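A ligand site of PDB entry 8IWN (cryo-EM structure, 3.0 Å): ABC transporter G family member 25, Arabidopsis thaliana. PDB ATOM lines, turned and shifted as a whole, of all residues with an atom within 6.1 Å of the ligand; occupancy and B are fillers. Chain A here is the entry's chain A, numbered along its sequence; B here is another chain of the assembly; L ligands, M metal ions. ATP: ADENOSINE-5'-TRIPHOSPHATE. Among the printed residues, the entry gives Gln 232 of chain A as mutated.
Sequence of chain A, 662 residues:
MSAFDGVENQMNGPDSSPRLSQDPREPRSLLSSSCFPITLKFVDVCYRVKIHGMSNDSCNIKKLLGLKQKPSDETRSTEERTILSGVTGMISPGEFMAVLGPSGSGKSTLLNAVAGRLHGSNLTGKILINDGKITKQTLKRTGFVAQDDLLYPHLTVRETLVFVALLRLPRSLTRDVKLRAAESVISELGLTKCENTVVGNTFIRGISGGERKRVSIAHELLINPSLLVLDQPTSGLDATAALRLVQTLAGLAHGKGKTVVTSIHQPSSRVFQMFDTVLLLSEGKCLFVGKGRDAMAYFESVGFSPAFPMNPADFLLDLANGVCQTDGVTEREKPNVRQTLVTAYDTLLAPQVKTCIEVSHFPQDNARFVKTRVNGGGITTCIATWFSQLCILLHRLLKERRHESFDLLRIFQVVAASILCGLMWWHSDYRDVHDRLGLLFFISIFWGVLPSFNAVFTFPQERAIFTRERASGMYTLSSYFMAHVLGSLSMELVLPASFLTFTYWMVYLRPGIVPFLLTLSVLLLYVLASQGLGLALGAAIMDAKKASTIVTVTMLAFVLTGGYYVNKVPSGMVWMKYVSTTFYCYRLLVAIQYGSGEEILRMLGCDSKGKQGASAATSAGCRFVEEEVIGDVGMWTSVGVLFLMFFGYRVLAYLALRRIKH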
ATOM      1  N   TYR A  47     -37.592 -31.632 -24.105  1.00  0.00           N
ATOM      2  CA  TYR A  47     -38.034 -30.291 -23.732  1.00  0.00           C
ATOM      3  C   TYR A  47     -38.464 -29.557 -24.990  1.00  0.00           C
ATOM      4  O   TYR A  47     -37.624 -29.216 -25.812  1.00  0.00           O
ATOM      5  CB  TYR A  47     -36.934 -29.525 -23.019  1.00  0.00           C
ATOM      6  CG  TYR A  47     -37.385 -28.217 -22.439  1.00  0.00           C
ATOM      7  CD1 TYR A  47     -38.144 -28.184 -21.305  1.00  0.00           C
ATOM      8  CD2 TYR A  47     -37.033 -27.028 -23.017  1.00  0.00           C
ATOM      9  CE1 TYR A  47     -38.543 -27.013 -20.764  1.00  0.00           C
ATOM     10  CE2 TYR A  47     -37.437 -25.838 -22.489  1.00  0.00           C
ATOM     11  CZ  TYR A  47     -38.190 -25.845 -21.361  1.00  0.00           C
ATOM     12  OH  TYR A  47     -38.620 -24.675 -20.800  1.00  0.00           O
ATOM     13  N   VAL A  49     -40.657 -26.205 -26.681  1.00  0.00           N
ATOM     14  CA  VAL A  49     -41.071 -24.855 -26.349  1.00  0.00           C
ATOM     15  C   VAL A  49     -41.868 -24.317 -27.528  1.00  0.00           C
ATOM     16  O   VAL A  49     -41.775 -24.831 -28.648  1.00  0.00           O
ATOM     17  CB  VAL A  49     -39.880 -23.943 -25.996  1.00  0.00           C
ATOM     18  CG1 VAL A  49     -39.178 -23.463 -27.226  1.00  0.00           C
ATOM     19  CG2 VAL A  49     -40.290 -22.816 -25.089  1.00  0.00           C
ATOM     20  N   LYS A  50     -42.705 -23.326 -27.262  1.00  0.00           N
ATOM     21  CA  LYS A  50     -43.614 -22.754 -28.248  1.00  0.00           C
ATOM     22  C   LYS A  50     -43.139 -21.353 -28.591  1.00  0.00           C
ATOM     23  O   LYS A  50     -43.113 -20.469 -27.733  1.00  0.00           O
ATOM     24  CB  LYS A  50     -45.041 -22.746 -27.703  1.00  0.00           C
ATOM     25  CG  LYS A  50     -46.081 -22.339 -28.704  1.00  0.00           C
ATOM     26  CD  LYS A  50     -47.465 -22.475 -28.089  1.00  0.00           C
ATOM     27  CE  LYS A  50     -48.109 -23.793 -28.504  1.00  0.00           C
ATOM     28  NZ  LYS A  50     -47.551 -24.974 -27.795  1.00  0.00           N
ATOM     29  N   ILE A  51     -42.783 -21.149 -29.857  1.00  0.00           N
ATOM     30  CA  ILE A  51     -42.138 -19.919 -30.274  1.00  0.00           C
ATOM     31  C   ILE A  51     -43.138 -18.866 -30.718  1.00  0.00           C
ATOM     32  O   ILE A  51     -44.274 -19.170 -31.080  1.00  0.00           O
ATOM     33  CB  ILE A  51     -41.137 -20.217 -31.406  1.00  0.00           C
ATOM     34  CG1 ILE A  51     -40.279 -18.989 -31.710  1.00  0.00           C
ATOM     35  CG2 ILE A  51     -41.848 -20.742 -32.654  1.00  0.00           C
ATOM     36  CD1 ILE A  51     -39.080 -19.319 -32.534  1.00  0.00           C
ATOM     37  N   ARG A  81     -40.565 -25.890 -31.111  1.00  0.00           N
ATOM     38  CA  ARG A  81     -39.144 -26.088 -31.302  1.00  0.00           C
ATOM     39  C   ARG A  81     -38.649 -27.068 -30.252  1.00  0.00           C
ATOM     40  O   ARG A  81     -38.953 -26.901 -29.076  1.00  0.00           O
ATOM     41  CB  ARG A  81     -38.405 -24.754 -31.199  1.00  0.00           C
ATOM     42  CG  ARG A  81     -36.923 -24.838 -31.443  1.00  0.00           C
ATOM     43  CD  ARG A  81     -36.281 -23.467 -31.351  1.00  0.00           C
ATOM     44  NE  ARG A  81     -34.823 -23.545 -31.371  1.00  0.00           N
ATOM     45  CZ  ARG A  81     -34.021 -22.496 -31.271  1.00  0.00           C
ATOM     46  NH1 ARG A  81     -34.540 -21.286 -31.137  1.00  0.00           N
ATOM     47  NH2 ARG A  81     -32.716 -22.652 -31.289  1.00  0.00           N
ATOM     48  N   ILE A  83     -35.874 -28.416 -28.017  1.00  0.00           N
ATOM     49  CA  ILE A  83     -34.603 -27.977 -27.468  1.00  0.00           C
ATOM     50  C   ILE A  83     -33.749 -29.149 -27.030  1.00  0.00           C
ATOM     51  O   ILE A  83     -32.570 -29.217 -27.350  1.00  0.00           O
ATOM     52  CB  ILE A  83     -34.851 -26.982 -26.315  1.00  0.00           C
ATOM     53  CG1 ILE A  83     -35.519 -25.720 -26.844  1.00  0.00           C
ATOM     54  CG2 ILE A  83     -33.571 -26.622 -25.647  1.00  0.00           C
ATOM     55  CD1 ILE A  83     -36.009 -24.836 -25.771  1.00  0.00           C
ATOM     56  N   GLY A 101     -20.244 -28.868 -25.624  1.00  0.00           N
ATOM     57  CA  GLY A 101     -21.107 -28.674 -26.759  1.00  0.00           C
ATOM     58  C   GLY A 101     -21.028 -27.283 -27.334  1.00  0.00           C
ATOM     59  O   GLY A 101     -20.434 -26.383 -26.749  1.00  0.00           O
ATOM     60  N   PRO A 102     -21.621 -27.080 -28.508  1.00  0.00           N
ATOM     61  CA  PRO A 102     -21.648 -25.743 -29.105  1.00  0.00           C
ATOM     62  C   PRO A 102     -22.582 -24.770 -28.412  1.00  0.00           C
ATOM     63  O   PRO A 102     -23.132 -25.065 -27.358  1.00  0.00           O
ATOM     64  CB  PRO A 102     -22.120 -26.038 -30.530  1.00  0.00           C
ATOM     65  CG  PRO A 102     -21.753 -27.416 -30.776  1.00  0.00           C
ATOM     66  CD  PRO A 102     -21.941 -28.117 -29.489  1.00  0.00           C
ATOM     67  N   SER A 103     -22.744 -23.589 -28.990  1.00  0.00           N
ATOM     68  CA  SER A 103     -23.663 -22.604 -28.455  1.00  0.00           C
ATOM     69  C   SER A 103     -25.068 -22.907 -28.939  1.00  0.00           C
ATOM     70  O   SER A 103     -25.299 -23.103 -30.123  1.00  0.00           O
ATOM     71  CB  SER A 103     -23.261 -21.195 -28.882  1.00  0.00           C
ATOM     72  OG  SER A 103     -21.990 -20.855 -28.403  1.00  0.00           O
ATOM     73  N   GLY A 104     -26.014 -22.942 -28.010  1.00  0.00           N
ATOM     74  CA  GLY A 104     -27.370 -23.274 -28.340  1.00  0.00           C
ATOM     75  C   GLY A 104     -27.665 -24.748 -28.382  1.00  0.00           C
ATOM     76  O   GLY A 104     -28.771 -25.121 -28.770  1.00  0.00           O
ATOM     77  N   SER A 105     -26.723 -25.600 -27.990  1.00  0.00           N
ATOM     78  CA  SER A 105     -26.961 -27.031 -28.066  1.00  0.00           C
ATOM     79  C   SER A 105     -27.834 -27.545 -26.947  1.00  0.00           C
ATOM     80  O   SER A 105     -28.288 -28.691 -27.004  1.00  0.00           O
ATOM     81  CB  SER A 105     -25.638 -27.784 -28.080  1.00  0.00           C
ATOM     82  OG  SER A 105     -24.986 -27.629 -26.847  1.00  0.00           O
ATOM     83  N   GLY A 106     -28.083 -26.731 -25.931  1.00  0.00           N
ATOM     84  CA  GLY A 106     -29.038 -27.052 -24.900  1.00  0.00           C
ATOM     85  C   GLY A 106     -28.458 -27.406 -23.565  1.00  0.00           C
ATOM     86  O   GLY A 106     -29.199 -27.913 -22.720  1.00  0.00           O
ATOM     87  N   LYS A 107     -27.199 -27.135 -23.316  1.00  0.00           N
ATOM     88  CA  LYS A 107     -26.546 -27.653 -22.131  1.00  0.00           C
ATOM     89  C   LYS A 107     -26.729 -26.775 -20.906  1.00  0.00           C
ATOM     90  O   LYS A 107     -26.254 -27.153 -19.845  1.00  0.00           O
ATOM     91  CB  LYS A 107     -25.062 -27.874 -22.410  1.00  0.00           C
ATOM     92  CG  LYS A 107     -24.310 -26.656 -22.780  1.00  0.00           C
ATOM     93  CD  LYS A 107     -22.930 -26.991 -23.210  1.00  0.00           C
ATOM     94  CE  LYS A 107     -22.190 -25.738 -23.489  1.00  0.00           C
ATOM     95  NZ  LYS A 107     -22.826 -25.040 -24.613  1.00  0.00           N
ATOM     96  N   SER A 108     -27.389 -25.643 -21.006  1.00  0.00           N
ATOM     97  CA  SER A 108     -27.841 -24.930 -19.832  1.00  0.00           C
ATOM     98  C   SER A 108     -29.314 -25.114 -19.560  1.00  0.00           C
ATOM     99  O   SER A 108     -29.798 -24.619 -18.560  1.00  0.00           O
ATOM    100  CB  SER A 108     -27.573 -23.443 -19.955  1.00  0.00           C
ATOM    101  OG  SER A 108     -28.194 -22.752 -18.906  1.00  0.00           O
ATOM    102  N   THR A 109     -30.031 -25.744 -20.478  1.00  0.00           N
ATOM    103  CA  THR A 109     -31.370 -26.233 -20.201  1.00  0.00           C
ATOM    104  C   THR A 109     -31.307 -27.594 -19.513  1.00  0.00           C
ATOM    105  O   THR A 109     -32.130 -27.898 -18.657  1.00  0.00           O
ATOM    106  CB  THR A 109     -32.165 -26.281 -21.513  1.00  0.00           C
ATOM    107  OG1 THR A 109     -32.317 -24.959 -22.038  1.00  0.00           O
ATOM    108  CG2 THR A 109     -33.533 -26.859 -21.354  1.00  0.00           C
ATOM    109  N   LEU A 110     -30.311 -28.404 -19.851  1.00  0.00           N
ATOM    110  CA  LEU A 110     -30.155 -29.706 -19.204  1.00  0.00           C
ATOM    111  C   LEU A 110     -29.674 -29.562 -17.772  1.00  0.00           C
ATOM    112  O   LEU A 110     -30.135 -30.292 -16.882  1.00  0.00           O
ATOM    113  CB  LEU A 110     -29.195 -30.561 -20.005  1.00  0.00           C
ATOM    114  CG  LEU A 110     -28.885 -31.960 -19.504  1.00  0.00           C
ATOM    115  CD1 LEU A 110     -30.119 -32.801 -19.489  1.00  0.00           C
ATOM    116  CD2 LEU A 110     -27.864 -32.561 -20.385  1.00  0.00           C
ATOM    117  N   GLN A 147     -25.326 -18.898 -14.337  1.00  0.00           N
ATOM    118  CA  GLN A 147     -24.399 -18.273 -15.263  1.00  0.00           C
ATOM    119  C   GLN A 147     -24.327 -16.757 -15.105  1.00  0.00           C
ATOM    120  O   GLN A 147     -23.253 -16.189 -15.307  1.00  0.00           O
ATOM    121  CB  GLN A 147     -24.792 -18.632 -16.701  1.00  0.00           C
ATOM    122  CG  GLN A 147     -23.815 -18.211 -17.763  1.00  0.00           C
ATOM    123  CD  GLN A 147     -24.234 -18.645 -19.136  1.00  0.00           C
ATOM    124  OE1 GLN A 147     -25.244 -19.308 -19.304  1.00  0.00           O
ATOM    125  NE2 GLN A 147     -23.474 -18.248 -20.136  1.00  0.00           N
ATOM    126  N   ASP A 231     -22.604 -23.816 -13.989  1.00  0.00           N
ATOM    127  CA  ASP A 231     -22.929 -23.458 -15.358  1.00  0.00           C
ATOM    128  C   ASP A 231     -21.873 -22.467 -15.854  1.00  0.00           C
ATOM    129  O   ASP A 231     -21.975 -21.281 -15.593  1.00  0.00           O
ATOM    130  CB  ASP A 231     -24.316 -22.860 -15.431  1.00  0.00           C
ATOM    131  CG  ASP A 231     -24.850 -22.773 -16.836  1.00  0.00           C
ATOM    132  OD1 ASP A 231     -24.171 -23.183 -17.786  1.00  0.00           O
ATOM    133  OD2 ASP A 231     -25.994 -22.283 -16.985  1.00  0.00           O
ATOM    134  N   GLN A 232     -20.885 -22.982 -16.577  1.00  0.00           N
ATOM    135  CA  GLN A 232     -19.712 -22.292 -17.107  1.00  0.00           C
ATOM    136  C   GLN A 232     -18.953 -21.517 -16.049  1.00  0.00           C
ATOM    137  O   GLN A 232     -19.003 -20.283 -16.041  1.00  0.00           O
ATOM    138  CB  GLN A 232     -20.110 -21.348 -18.237  1.00  0.00           C
ATOM    139  CG  GLN A 232     -20.668 -22.035 -19.438  1.00  0.00           C
ATOM    140  CD  GLN A 232     -21.023 -21.078 -20.523  1.00  0.00           C
ATOM    141  OE1 GLN A 232     -20.745 -19.892 -20.422  1.00  0.00           O
ATOM    142  NE2 GLN A 232     -21.748 -21.552 -21.509  1.00  0.00           N
ATOM    143  N   HIS A 265     -16.538 -24.335 -21.742  1.00  0.00           N
ATOM    144  CA  HIS A 265     -16.428 -24.011 -23.158  1.00  0.00           C
ATOM    145  C   HIS A 265     -15.059 -24.249 -23.798  1.00  0.00           C
ATOM    146  O   HIS A 265     -14.979 -24.993 -24.771  1.00  0.00           O
ATOM    147  CB  HIS A 265     -16.879 -22.595 -23.471  1.00  0.00           C
ATOM    148  CG  HIS A 265     -18.304 -22.526 -23.886  1.00  0.00           C
ATOM    149  ND1 HIS A 265     -18.778 -23.223 -24.976  1.00  0.00           N
ATOM    150  CD2 HIS A 265     -19.335 -21.806 -23.419  1.00  0.00           C
ATOM    151  CE1 HIS A 265     -20.063 -22.967 -25.133  1.00  0.00           C
ATOM    152  NE2 HIS A 265     -20.426 -22.109 -24.205  1.00  0.00           N
ATOM    153  N   CYS B 194     -31.950 -18.507 -34.389  1.00  0.00           N
ATOM    154  CA  CYS B 194     -32.621 -17.841 -33.292  1.00  0.00           C
ATOM    155  C   CYS B 194     -33.060 -16.442 -33.696  1.00  0.00           C
ATOM    156  O   CYS B 194     -33.301 -15.617 -32.827  1.00  0.00           O
ATOM    157  CB  CYS B 194     -31.696 -17.764 -32.091  1.00  0.00           C
ATOM    158  SG  CYS B 194     -30.225 -16.807 -32.390  1.00  0.00           S
ATOM    159  N   THR B 197     -36.490 -15.623 -32.507  1.00  0.00           N
ATOM    160  CA  THR B 197     -36.618 -15.820 -31.080  1.00  0.00           C
ATOM    161  C   THR B 197     -36.408 -14.493 -30.375  1.00  0.00           C
ATOM    162  O   THR B 197     -35.544 -13.715 -30.765  1.00  0.00           O
ATOM    163  CB  THR B 197     -35.593 -16.842 -30.606  1.00  0.00           C
ATOM    164  OG1 THR B 197     -35.742 -18.032 -31.371  1.00  0.00           O
ATOM    165  CG2 THR B 197     -35.795 -17.191 -29.147  1.00  0.00           C
ATOM    166  N   ARG B 205     -37.408 -15.736 -20.457  1.00  0.00           N
ATOM    167  CA  ARG B 205     -36.414 -16.645 -21.009  1.00  0.00           C
ATOM    168  C   ARG B 205     -36.418 -16.548 -22.528  1.00  0.00           C
ATOM    169  O   ARG B 205     -37.447 -16.736 -23.169  1.00  0.00           O
ATOM    170  CB  ARG B 205     -36.659 -18.061 -20.523  1.00  0.00           C
ATOM    171  CG  ARG B 205     -35.734 -19.088 -21.118  1.00  0.00           C
ATOM    172  CD  ARG B 205     -34.259 -18.774 -20.875  1.00  0.00           C
ATOM    173  NE  ARG B 205     -33.414 -19.812 -21.454  1.00  0.00           N
ATOM    174  CZ  ARG B 205     -32.121 -19.670 -21.726  1.00  0.00           C
ATOM    175  NH1 ARG B 205     -31.442 -20.681 -22.244  1.00  0.00           N
ATOM    176  NH2 ARG B 205     -31.519 -18.517 -21.506  1.00  0.00           N
ATOM    177  N   GLY B 206     -35.250 -16.232 -23.095  1.00  0.00           N
ATOM    178  CA  GLY B 206     -35.086 -16.058 -24.522  1.00  0.00           C
ATOM    179  C   GLY B 206     -33.871 -16.763 -25.078  1.00  0.00           C
ATOM    180  O   GLY B 206     -33.733 -17.967 -24.889  1.00  0.00           O
ATOM    181  N   ILE B 207     -32.985 -16.034 -25.741  1.00  0.00           N
ATOM    182  CA  ILE B 207     -31.808 -16.603 -26.400  1.00  0.00           C
ATOM    183  C   ILE B 207     -30.726 -16.949 -25.381  1.00  0.00           C
ATOM    184  O   ILE B 207     -30.808 -16.572 -24.215  1.00  0.00           O
ATOM    185  CB  ILE B 207     -31.276 -15.656 -27.491  1.00  0.00           C
ATOM    186  CG1 ILE B 207     -30.946 -14.287 -26.914  1.00  0.00           C
ATOM    187  CG2 ILE B 207     -32.250 -15.514 -28.608  1.00  0.00           C
ATOM    188  CD1 ILE B 207     -30.297 -13.380 -27.888  1.00  0.00           C
ATOM    189  N   SER B 208     -29.696 -17.657 -25.838  1.00  0.00           N
ATOM    190  CA  SER B 208     -28.606 -18.128 -25.001  1.00  0.00           C
ATOM    191  C   SER B 208     -27.703 -16.984 -24.582  1.00  0.00           C
ATOM    192  O   SER B 208     -27.881 -15.840 -24.959  1.00  0.00           O
ATOM    193  CB  SER B 208     -27.772 -19.141 -25.757  1.00  0.00           C
ATOM    194  OG  SER B 208     -28.553 -20.234 -26.114  1.00  0.00           O
ATOM    195  N   GLY B 209     -26.679 -17.321 -23.815  1.00  0.00           N
ATOM    196  CA  GLY B 209     -25.685 -16.344 -23.415  1.00  0.00           C
ATOM    197  C   GLY B 209     -24.617 -16.164 -24.465  1.00  0.00           C
ATOM    198  O   GLY B 209     -24.022 -15.090 -24.562  1.00  0.00           O
ATOM    199  N   GLY B 210     -24.346 -17.205 -25.233  1.00  0.00           N
ATOM    200  CA  GLY B 210     -23.415 -17.099 -26.341  1.00  0.00           C
ATOM    201  C   GLY B 210     -24.035 -16.575 -27.608  1.00  0.00           C
ATOM    202  O   GLY B 210     -23.310 -16.162 -28.507  1.00  0.00           O
ATOM    203  N   GLU B 211     -25.358 -16.601 -27.704  1.00  0.00           N
ATOM    204  CA  GLU B 211     -26.065 -15.933 -28.786  1.00  0.00           C
ATOM    205  C   GLU B 211     -26.304 -14.471 -28.462  1.00  0.00           C
ATOM    206  O   GLU B 211     -26.352 -13.643 -29.368  1.00  0.00           O
ATOM    207  CB  GLU B 211     -27.382 -16.618 -29.062  1.00  0.00           C
ATOM    208  CG  GLU B 211     -27.224 -18.025 -29.563  1.00  0.00           C
ATOM    209  CD  GLU B 211     -28.536 -18.726 -29.773  1.00  0.00           C
ATOM    210  OE1 GLU B 211     -29.566 -18.162 -29.396  1.00  0.00           O
ATOM    211  OE2 GLU B 211     -28.532 -19.842 -30.333  1.00  0.00           O
ATOM    212  N   ARG B 214     -23.111 -12.501 -29.416  1.00  0.00           N
ATOM    213  CA  ARG B 214     -22.918 -12.241 -30.834  1.00  0.00           C
ATOM    214  C   ARG B 214     -23.930 -11.265 -31.408  1.00  0.00           C
ATOM    215  O   ARG B 214     -23.679 -10.709 -32.465  1.00  0.00           O
ATOM    216  CB  ARG B 214     -22.960 -13.549 -31.613  1.00  0.00           C
ATOM    217  CG  ARG B 214     -21.775 -14.431 -31.337  1.00  0.00           C
ATOM    218  CD  ARG B 214     -21.876 -15.748 -32.055  1.00  0.00           C
ATOM    219  NE  ARG B 214     -22.912 -16.589 -31.471  1.00  0.00           N
ATOM    220  CZ  ARG B 214     -23.325 -17.716 -32.017  1.00  0.00           C
ATOM    221  NH1 ARG B 214     -22.812 -18.126 -33.152  1.00  0.00           N
ATOM    222  NH2 ARG B 214     -24.272 -18.426 -31.427  1.00  0.00           N
ATOM    223  N   GLY B 236     -17.907 -17.171 -23.419  1.00  0.00           N
ATOM    224  CA  GLY B 236     -19.212 -17.743 -23.652  1.00  0.00           C
ATOM    225  C   GLY B 236     -19.375 -18.362 -25.006  1.00  0.00           C
ATOM    226  O   GLY B 236     -20.486 -18.744 -25.363  1.00  0.00           O
HETATM  227  PG  ATP L   1     -24.552 -21.216 -24.603  1.00  0.00           P
HETATM  228  O1G ATP L   1     -24.817 -20.701 -23.223  1.00  0.00           O
HETATM  229  O2G ATP L   1     -23.410 -22.162 -24.690  1.00  0.00           O
HETATM  230  O3G ATP L   1     -24.488 -20.143 -25.641  1.00  0.00           O
HETATM  231  PB  ATP L   1     -26.463 -23.305 -24.297  1.00  0.00           P
HETATM  232  O1B ATP L   1     -26.437 -23.009 -22.853  1.00  0.00           O
HETATM  233  O2B ATP L   1     -25.726 -24.491 -24.806  1.00  0.00           O
HETATM  234  O3B ATP L   1     -25.832 -22.055 -25.066  1.00  0.00           O
HETATM  235  PA  ATP L   1     -29.328 -23.084 -23.996  1.00  0.00           P
HETATM  236  O1A ATP L   1     -29.939 -24.242 -23.304  1.00  0.00           O
HETATM  237  O2A ATP L   1     -29.142 -21.798 -23.277  1.00  0.00           O
HETATM  238  O3A ATP L   1     -27.986 -23.478 -24.784  1.00  0.00           O
HETATM  239  O5' ATP L   1     -30.361 -22.837 -25.181  1.00  0.00           O
HETATM  240  C5' ATP L   1     -30.459 -23.756 -26.250  1.00  0.00           C
HETATM  241  C4' ATP L   1     -31.355 -23.184 -27.325  1.00  0.00           C
HETATM  242  O4' ATP L   1     -32.679 -23.081 -26.829  1.00  0.00           O
HETATM  243  C3' ATP L   1     -30.942 -21.786 -27.681  1.00  0.00           C
HETATM  244  O3' ATP L   1     -30.819 -21.711 -29.093  1.00  0.00           O
HETATM  245  C2' ATP L   1     -32.068 -20.882 -27.260  1.00  0.00           C
HETATM  246  O2' ATP L   1     -32.274 -19.910 -28.282  1.00  0.00           O
HETATM  247  C1' ATP L   1     -33.227 -21.833 -27.193  1.00  0.00           C
HETATM  248  N9  ATP L   1     -34.172 -21.449 -26.139  1.00  0.00           N
HETATM  249  C8  ATP L   1     -33.982 -21.580 -24.827  1.00  0.00           C
HETATM  250  N7  ATP L   1     -35.059 -21.143 -24.143  1.00  0.00           N
HETATM  251  C5  ATP L   1     -35.956 -20.717 -25.039  1.00  0.00           C
HETATM  252  C6  ATP L   1     -37.309 -20.139 -25.005  1.00  0.00           C
HETATM  253  N6  ATP L   1     -37.905 -19.921 -23.822  1.00  0.00           N
HETATM  254  N1  ATP L   1     -37.901 -19.838 -26.163  1.00  0.00           N
HETATM  255  C2  ATP L   1     -37.306 -20.061 -27.339  1.00  0.00           C
HETATM  256  N3  ATP L   1     -36.084 -20.591 -27.446  1.00  0.00           N
HETATM  257  C4  ATP L   1     -35.376 -20.924 -26.360  1.00  0.00           C
HETATM  258 MG    MG M   1     -27.142 -20.086 -21.510  1.00  0.00          MG
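The backbone carbonyl oxygen (O) of Pro 102 is in hydrogen-bond range of the side-chain hydroxyl (OG) of Ser 105 (3.2 Å). The side-chain carboxylate (OE1) of Glu 211 of chain B is in hydrogen-bond range of the side-chain sulfur (SG) of Cys 194 of chain B, 3.4 Å away. The side-chain amide nitrogen (NE2) of Gln 232 sits at hydrogen-bond distance from a ring nitrogen (NE2) of His 265. NE2 of Gln 147 sits at hydrogen-bond distance from OE1 of Gln 232 (3.2 Å). The side-chain amino group (NZ) of Lys 107 is in hydrogen-bond range of the backbone carbonyl oxygen (O) of Pro 102 (2.8 Å). The backbone NH (N) of Ile 83 sits at hydrogen-bond distance from the backbone carbonyl oxygen (O) of Tyr 47 (2.9 Å). The backbone carbonyl oxygen (O) of Val 49 is in hydrogen-bond range of the backbone NH (N) of Arg 81 (2.9 Å). The guanidinium group (NH1) of Arg 81 is in hydrogen-bond range of the side-chain hydroxyl (OG1) of Thr 197 of chain B (3.5 Å).
An oxygen (O2A) of the ligand is in salt-bridge range of the guanidinium group of Arg 205 of chain B (2.8 Å). The side-chain amino group of Lys 107 is in salt-bridge range of an oxygen (O2G) of the ligand (2.9 Å). The side-chain carboxylate (OE2) of Glu 211 of chain B sits at hydrogen-bond distance from an oxygen (O3') of the ligand, at 3.2 Å. N of Gly 106 sits at hydrogen-bond distance from O2B of the ligand, at 3.4 Å. OG of Ser 208 of chain B lies close to O2A of the ligand, 3.3 Å away. O1A of the ligand lies within hydrogen-bond range of N of Thr 109. A ring nitrogen (NE2) of His 265 is in hydrogen-bond range of an oxygen (O2G) of the ligand (3.0 Å). NH2 of Arg 81 sits at hydrogen-bond distance from O3' of the ligand. The backbone carbonyl oxygen (O) of Arg 205 of chain B is in hydrogen-bond range of a nitrogen (N6) of the ligand (3.3 Å). N of Ser 108 sits close to O1B of the ligand. N of Gly 210 of chain B is in hydrogen-bond range of O3G of the ligand, 3.0 Å away. The side-chain hydroxyl (OG1) of Thr 109 sits at hydrogen-bond distance from an oxygen (O1A) of the ligand, at 2.8 Å. O2B of the ligand lies close to N of Lys 107, 3.4 Å away. The backbone NH (N) of Gly 104 sits at hydrogen-bond distance from an oxygen (O3B) of the ligand (3.1 Å).
Merely in contact with the ligand: Val 49, Ile 83, Pro 102, Ser 103, Ser 105, Gln 232, Thr 197 of chain B, Gly 206 of chain B, Ile 207 of chain B and Gly 209 of chain B. Hydrophobic or aromatic side chains within 4 Å of the ligand: Val 49, Ile 83 and His 265.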
